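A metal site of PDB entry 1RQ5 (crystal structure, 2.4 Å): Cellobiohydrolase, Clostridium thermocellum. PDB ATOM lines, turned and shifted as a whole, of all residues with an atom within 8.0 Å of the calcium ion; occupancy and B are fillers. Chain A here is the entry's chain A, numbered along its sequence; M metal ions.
The backbone NH of Met 217 is in hydrogen-bond range of the side-chain carboxylate of Asp 228 (2.9 Å). The side-chain carboxylate (OD2) of Asp 228 lies close to the backbone NH (N) of Gly 215, 3.2 Å away. OD2 of Asp 214 lies close to O of Gln 222 (2.5 Å). N of Asp 228 is in hydrogen-bond range of O of Arg 213, 3.3 Å away. The side-chain carboxylate (OD1) of Asp 214 is in hydrogen-bond range of the backbone NH (N) of Gly 225. N of Gly 216 is in hydrogen-bond range of OD2 of Asp 228, at 3.2 Å. The backbone carbonyl oxygen (O) of Gln 222 is in hydrogen-bond range of the backbone NH (N) of Gly 215 (2.6 Å).
Merely in contact with the calcium ion: Gln 222. Within 4 Å of the calcium ion: Asp 214, Glu 221, Gln 222, Asn 224, Tyr 226, Asp 228 and Asp 231. Along chain A the residues within 4 Å of the calcium ion span positions 214 to 231.
The side-chain carboxylate (OD1) of Asp 231 binds the calcium ion, 2.4 Å away. The side-chain carboxylate (OD2) of Asp 214 is bound to the calcium ion. O of Glu 221 is bound to the calcium ion (2.5 Å). O of Tyr 226 is bound to the calcium ion (2.5 Å). OD1 of Asp 228 binds the calcium ion (2.7 Å). The calcium ion is bound by OD1 of Asn 224 (2.8 Å). The calcium ion has six donor atoms within binding distance.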
ATOM      1  N   PRO A 211      22.914  -4.922 -10.430  1.00  0.00           N
ATOM      2  CA  PRO A 211      21.966  -4.656 -11.510  1.00  0.00           C
ATOM      3  C   PRO A 211      21.387  -5.884 -12.215  1.00  0.00           C
ATOM      4  O   PRO A 211      20.516  -5.758 -13.066  1.00  0.00           O
ATOM      5  CB  PRO A 211      22.774  -3.799 -12.461  1.00  0.00           C
ATOM      6  CG  PRO A 211      24.128  -4.424 -12.351  1.00  0.00           C
ATOM      7  CD  PRO A 211      24.292  -4.609 -10.856  1.00  0.00           C
ATOM      8  N   TYR A 212      21.877  -7.057 -11.871  1.00  0.00           N
ATOM      9  CA  TYR A 212      21.381  -8.270 -12.496  1.00  0.00           C
ATOM     10  C   TYR A 212      20.023  -8.731 -11.965  1.00  0.00           C
ATOM     11  O   TYR A 212      19.404  -9.636 -12.519  1.00  0.00           O
ATOM     12  CB  TYR A 212      22.402  -9.381 -12.292  1.00  0.00           C
ATOM     13  CG  TYR A 212      23.790  -9.007 -12.782  1.00  0.00           C
ATOM     14  CD1 TYR A 212      24.072  -8.921 -14.144  1.00  0.00           C
ATOM     15  CD2 TYR A 212      24.815  -8.752 -11.869  1.00  0.00           C
ATOM     16  CE1 TYR A 212      25.350  -8.602 -14.597  1.00  0.00           C
ATOM     17  CE2 TYR A 212      26.097  -8.428 -12.310  1.00  0.00           C
ATOM     18  CZ  TYR A 212      26.364  -8.357 -13.676  1.00  0.00           C
ATOM     19  OH  TYR A 212      27.637  -8.072 -14.119  1.00  0.00           O
ATOM     20  N   ARG A 213      19.545  -8.101 -10.891  1.00  0.00           N
ATOM     21  CA  ARG A 213      18.282  -8.508 -10.310  1.00  0.00           C
ATOM     22  C   ARG A 213      17.168  -7.500 -10.550  1.00  0.00           C
ATOM     23  O   ARG A 213      17.436  -6.335 -10.864  1.00  0.00           O
ATOM     24  CB  ARG A 213      18.444  -8.706  -8.809  1.00  0.00           C
ATOM     25  CG  ARG A 213      18.741  -7.432  -8.051  1.00  0.00           C
ATOM     26  CD  ARG A 213      18.785  -7.665  -6.569  1.00  0.00           C
ATOM     27  NE  ARG A 213      18.435  -6.435  -5.853  1.00  0.00           N
ATOM     28  CZ  ARG A 213      19.163  -5.317  -5.868  1.00  0.00           C
ATOM     29  NH1 ARG A 213      20.298  -5.275  -6.551  1.00  0.00           N
ATOM     30  NH2 ARG A 213      18.755  -4.257  -5.184  1.00  0.00           N
ATOM     31  N   ASP A 214      15.926  -7.973 -10.401  1.00  0.00           N
ATOM     32  CA  ASP A 214      14.727  -7.144 -10.544  1.00  0.00           C
ATOM     33  C   ASP A 214      14.887  -6.107  -9.426  1.00  0.00           C
ATOM     34  O   ASP A 214      15.118  -6.470  -8.259  1.00  0.00           O
ATOM     35  CB  ASP A 214      13.454  -7.988 -10.331  1.00  0.00           C
ATOM     36  CG  ASP A 214      12.152  -7.182 -10.544  1.00  0.00           C
ATOM     37  OD1 ASP A 214      11.114  -7.570  -9.964  1.00  0.00           O
ATOM     38  OD2 ASP A 214      12.128  -6.179 -11.275  1.00  0.00           O
ATOM     39  N   GLY A 215      14.778  -4.833  -9.762  1.00  0.00           N
ATOM     40  CA  GLY A 215      14.944  -3.809  -8.746  1.00  0.00           C
ATOM     41  C   GLY A 215      16.393  -3.405  -8.528  1.00  0.00           C
ATOM     42  O   GLY A 215      16.714  -2.687  -7.586  1.00  0.00           O
ATOM     43  N   GLY A 216      17.275  -3.868  -9.412  1.00  0.00           N
ATOM     44  CA  GLY A 216      18.682  -3.524  -9.274  1.00  0.00           C
ATOM     45  C   GLY A 216      19.096  -2.224  -9.944  1.00  0.00           C
ATOM     46  O   GLY A 216      20.166  -1.680  -9.639  1.00  0.00           O
ATOM     47  N   MET A 217      18.251  -1.719 -10.844  1.00  0.00           N
ATOM     48  CA  MET A 217      18.525  -0.482 -11.561  1.00  0.00           C
ATOM     49  C   MET A 217      17.384   0.508 -11.408  1.00  0.00           C
ATOM     50  O   MET A 217      16.216   0.118 -11.347  1.00  0.00           O
ATOM     51  CB  MET A 217      18.738  -0.761 -13.045  1.00  0.00           C
ATOM     52  CG  MET A 217      19.993  -1.544 -13.341  1.00  0.00           C
ATOM     53  SD  MET A 217      19.838  -2.387 -14.903  1.00  0.00           S
ATOM     54  CE  MET A 217      20.030  -1.032 -16.049  1.00  0.00           C
ATOM     55  N   ILE A 219      15.406   2.078 -13.049  1.00  0.00           N
ATOM     56  CA  ILE A 219      14.662   2.191 -14.284  1.00  0.00           C
ATOM     57  C   ILE A 219      13.194   1.909 -13.975  1.00  0.00           C
ATOM     58  O   ILE A 219      12.870   1.309 -12.951  1.00  0.00           O
ATOM     59  CB  ILE A 219      15.179   1.199 -15.321  1.00  0.00           C
ATOM     60  CG1 ILE A 219      15.047  -0.223 -14.773  1.00  0.00           C
ATOM     61  CG2 ILE A 219      16.653   1.530 -15.655  1.00  0.00           C
ATOM     62  CD1 ILE A 219      15.484  -1.296 -15.754  1.00  0.00           C
ATOM     63  N   PRO A 220      12.286   2.325 -14.878  1.00  0.00           N
ATOM     64  CA  PRO A 220      10.850   2.102 -14.681  1.00  0.00           C
ATOM     65  C   PRO A 220      10.441   0.638 -14.562  1.00  0.00           C
ATOM     66  O   PRO A 220       9.376   0.346 -14.019  1.00  0.00           O
ATOM     67  CB  PRO A 220      10.225   2.768 -15.915  1.00  0.00           C
ATOM     68  CG  PRO A 220      11.230   3.740 -16.348  1.00  0.00           C
ATOM     69  CD  PRO A 220      12.522   2.998 -16.154  1.00  0.00           C
ATOM     70  N   GLU A 221      11.263  -0.290 -15.059  1.00  0.00           N
ATOM     71  CA  GLU A 221      10.942  -1.723 -14.950  1.00  0.00           C
ATOM     72  C   GLU A 221      11.472  -2.288 -13.636  1.00  0.00           C
ATOM     73  O   GLU A 221      11.641  -3.482 -13.504  1.00  0.00           O
ATOM     74  CB  GLU A 221      11.549  -2.540 -16.108  1.00  0.00           C
ATOM     75  CG  GLU A 221      11.038  -2.186 -17.499  1.00  0.00           C
ATOM     76  CD  GLU A 221      11.650  -0.890 -18.067  1.00  0.00           C
ATOM     77  OE1 GLU A 221      12.730  -0.443 -17.605  1.00  0.00           O
ATOM     78  OE2 GLU A 221      11.062  -0.330 -19.002  1.00  0.00           O
ATOM     79  N   GLN A 222      11.728  -1.431 -12.659  1.00  0.00           N
ATOM     80  CA  GLN A 222      12.229  -1.844 -11.351  1.00  0.00           C
ATOM     81  C   GLN A 222      11.635  -3.096 -10.695  1.00  0.00           C
ATOM     82  O   GLN A 222      12.382  -3.912 -10.170  1.00  0.00           O
ATOM     83  CB  GLN A 222      12.084  -0.697 -10.359  1.00  0.00           C
ATOM     84  CG  GLN A 222      13.323   0.113 -10.194  1.00  0.00           C
ATOM     85  CD  GLN A 222      13.071   1.289  -9.296  1.00  0.00           C
ATOM     86  OE1 GLN A 222      12.110   2.020  -9.493  1.00  0.00           O
ATOM     87  NE2 GLN A 222      13.920   1.482  -8.298  1.00  0.00           N
ATOM     88  N   ASN A 223      10.322  -3.244 -10.647  1.00  0.00           N
ATOM     89  CA  ASN A 223       9.784  -4.448 -10.024  1.00  0.00           C
ATOM     90  C   ASN A 223       8.658  -5.054 -10.835  1.00  0.00           C
ATOM     91  O   ASN A 223       7.512  -5.086 -10.414  1.00  0.00           O
ATOM     92  CB  ASN A 223       9.331  -4.170  -8.586  1.00  0.00           C
ATOM     93  CG  ASN A 223      10.499  -4.076  -7.609  1.00  0.00           C
ATOM     94  OD1 ASN A 223      10.879  -2.979  -7.160  1.00  0.00           O
ATOM     95  ND2 ASN A 223      11.095  -5.215  -7.298  1.00  0.00           N
ATOM     96  N   ASN A 224       9.019  -5.550 -12.018  1.00  0.00           N
ATOM     97  CA  ASN A 224       8.061  -6.154 -12.924  1.00  0.00           C
ATOM     98  C   ASN A 224       8.336  -7.644 -13.061  1.00  0.00           C
ATOM     99  O   ASN A 224       7.892  -8.285 -14.024  1.00  0.00           O
ATOM    100  CB  ASN A 224       8.135  -5.442 -14.273  1.00  0.00           C
ATOM    101  CG  ASN A 224       9.360  -5.829 -15.099  1.00  0.00           C
ATOM    102  OD1 ASN A 224      10.304  -6.440 -14.612  1.00  0.00           O
ATOM    103  ND2 ASN A 224       9.326  -5.471 -16.367  1.00  0.00           N
ATOM    104  N   GLY A 225       9.081  -8.180 -12.105  1.00  0.00           N
ATOM    105  CA  GLY A 225       9.405  -9.591 -12.091  1.00  0.00           C
ATOM    106  C   GLY A 225      10.604 -10.062 -12.901  1.00  0.00           C
ATOM    107  O   GLY A 225      11.050 -11.192 -12.717  1.00  0.00           O
ATOM    108  N   TYR A 226      11.147  -9.208 -13.766  1.00  0.00           N
ATOM    109  CA  TYR A 226      12.277  -9.583 -14.608  1.00  0.00           C
ATOM    110  C   TYR A 226      13.606  -8.998 -14.161  1.00  0.00           C
ATOM    111  O   TYR A 226      13.650  -8.055 -13.393  1.00  0.00           O
ATOM    112  CB  TYR A 226      12.024  -9.159 -16.049  1.00  0.00           C
ATOM    113  CG  TYR A 226      10.704  -9.618 -16.592  1.00  0.00           C
ATOM    114  CD1 TYR A 226      10.178 -10.850 -16.237  1.00  0.00           C
ATOM    115  CD2 TYR A 226      10.003  -8.831 -17.517  1.00  0.00           C
ATOM    116  CE1 TYR A 226       8.982 -11.312 -16.785  1.00  0.00           C
ATOM    117  CE2 TYR A 226       8.806  -9.289 -18.075  1.00  0.00           C
ATOM    118  CZ  TYR A 226       8.312 -10.538 -17.697  1.00  0.00           C
ATOM    119  OH  TYR A 226       7.128 -11.024 -18.213  1.00  0.00           O
ATOM    120  N   PRO A 227      14.722  -9.573 -14.601  1.00  0.00           N
ATOM    121  CA  PRO A 227      15.995  -8.989 -14.169  1.00  0.00           C
ATOM    122  C   PRO A 227      16.169  -7.611 -14.823  1.00  0.00           C
ATOM    123  O   PRO A 227      16.010  -7.485 -16.031  1.00  0.00           O
ATOM    124  CB  PRO A 227      17.030 -10.023 -14.634  1.00  0.00           C
ATOM    125  CG  PRO A 227      16.238 -11.320 -14.579  1.00  0.00           C
ATOM    126  CD  PRO A 227      14.910 -10.925 -15.159  1.00  0.00           C
ATOM    127  N   ASP A 228      16.489  -6.584 -14.029  1.00  0.00           N
ATOM    128  CA  ASP A 228      16.618  -5.230 -14.568  1.00  0.00           C
ATOM    129  C   ASP A 228      17.553  -5.055 -15.757  1.00  0.00           C
ATOM    130  O   ASP A 228      17.173  -4.411 -16.741  1.00  0.00           O
ATOM    131  CB  ASP A 228      17.013  -4.247 -13.467  1.00  0.00           C
ATOM    132  CG  ASP A 228      15.843  -3.852 -12.582  1.00  0.00           C
ATOM    133  OD1 ASP A 228      14.911  -4.655 -12.440  1.00  0.00           O
ATOM    134  OD2 ASP A 228      15.831  -2.757 -11.999  1.00  0.00           O
ATOM    135  N   ILE A 229      18.762  -5.589 -15.692  1.00  0.00           N
ATOM    136  CA  ILE A 229      19.650  -5.438 -16.829  1.00  0.00           C
ATOM    137  C   ILE A 229      18.997  -6.013 -18.116  1.00  0.00           C
ATOM    138  O   ILE A 229      19.206  -5.489 -19.207  1.00  0.00           O
ATOM    139  CB  ILE A 229      21.030  -6.109 -16.599  1.00  0.00           C
ATOM    140  CG1 ILE A 229      22.031  -5.543 -17.604  1.00  0.00           C
ATOM    141  CG2 ILE A 229      20.935  -7.642 -16.801  1.00  0.00           C
ATOM    142  CD1 ILE A 229      23.437  -6.078 -17.447  1.00  0.00           C
ATOM    143  N   LEU A 230      18.197  -7.074 -18.008  1.00  0.00           N
ATOM    144  CA  LEU A 230      17.560  -7.599 -19.226  1.00  0.00           C
ATOM    145  C   LEU A 230      16.392  -6.709 -19.692  1.00  0.00           C
ATOM    146  O   LEU A 230      16.031  -6.706 -20.875  1.00  0.00           O
ATOM    147  CB  LEU A 230      17.068  -9.046 -19.015  1.00  0.00           C
ATOM    148  CG  LEU A 230      18.107 -10.169 -18.861  1.00  0.00           C
ATOM    149  CD1 LEU A 230      17.374 -11.510 -18.721  1.00  0.00           C
ATOM    150  CD2 LEU A 230      19.047 -10.187 -20.064  1.00  0.00           C
ATOM    151  N   ASP A 231      15.781  -5.967 -18.775  1.00  0.00           N
ATOM    152  CA  ASP A 231      14.684  -5.099 -19.173  1.00  0.00           C
ATOM    153  C   ASP A 231      15.233  -4.040 -20.138  1.00  0.00           C
ATOM    154  O   ASP A 231      14.592  -3.696 -21.132  1.00  0.00           O
ATOM    155  CB  ASP A 231      14.059  -4.432 -17.939  1.00  0.00           C
ATOM    156  CG  ASP A 231      13.107  -5.367 -17.190  1.00  0.00           C
ATOM    157  OD1 ASP A 231      13.255  -5.561 -15.963  1.00  0.00           O
ATOM    158  OD2 ASP A 231      12.206  -5.917 -17.838  1.00  0.00           O
ATOM    159  N   GLU A 232      16.434  -3.555 -19.839  1.00  0.00           N
ATOM    160  CA  GLU A 232      17.094  -2.554 -20.656  1.00  0.00           C
ATOM    161  C   GLU A 232      17.416  -3.161 -22.002  1.00  0.00           C
ATOM    162  O   GLU A 232      17.079  -2.615 -23.026  1.00  0.00           O
ATOM    163  CB  GLU A 232      18.397  -2.079 -20.010  1.00  0.00           C
ATOM    164  CG  GLU A 232      18.963  -0.802 -20.578  1.00  0.00           C
ATOM    165  CD  GLU A 232      18.006   0.366 -20.439  1.00  0.00           C
ATOM    166  OE1 GLU A 232      17.759   0.793 -19.283  1.00  0.00           O
ATOM    167  OE2 GLU A 232      17.490   0.842 -21.487  1.00  0.00           O
ATOM    168  N   TRP A 304      15.836 -15.041 -21.513  1.00  0.00           N
ATOM    169  CA  TRP A 304      14.489 -14.689 -21.080  1.00  0.00           C
ATOM    170  C   TRP A 304      13.531 -15.863 -20.950  1.00  0.00           C
ATOM    171  O   TRP A 304      12.402 -15.694 -20.523  1.00  0.00           O
ATOM    172  CB  TRP A 304      13.846 -13.696 -22.057  1.00  0.00           C
ATOM    173  CG  TRP A 304      14.187 -12.257 -21.824  1.00  0.00           C
ATOM    174  CD1 TRP A 304      15.201 -11.543 -22.382  1.00  0.00           C
ATOM    175  CD2 TRP A 304      13.459 -11.354 -20.995  1.00  0.00           C
ATOM    176  NE1 TRP A 304      15.155 -10.239 -21.945  1.00  0.00           N
ATOM    177  CE2 TRP A 304      14.097 -10.094 -21.098  1.00  0.00           C
ATOM    178  CE3 TRP A 304      12.336 -11.480 -20.162  1.00  0.00           C
ATOM    179  CZ2 TRP A 304      13.628  -8.954 -20.399  1.00  0.00           C
ATOM    180  CZ3 TRP A 304      11.880 -10.363 -19.473  1.00  0.00           C
ATOM    181  CH2 TRP A 304      12.531  -9.122 -19.594  1.00  0.00           C
HETATM  182 CA    CA M   1      12.771  -5.695 -13.609  1.00  0.00          CA
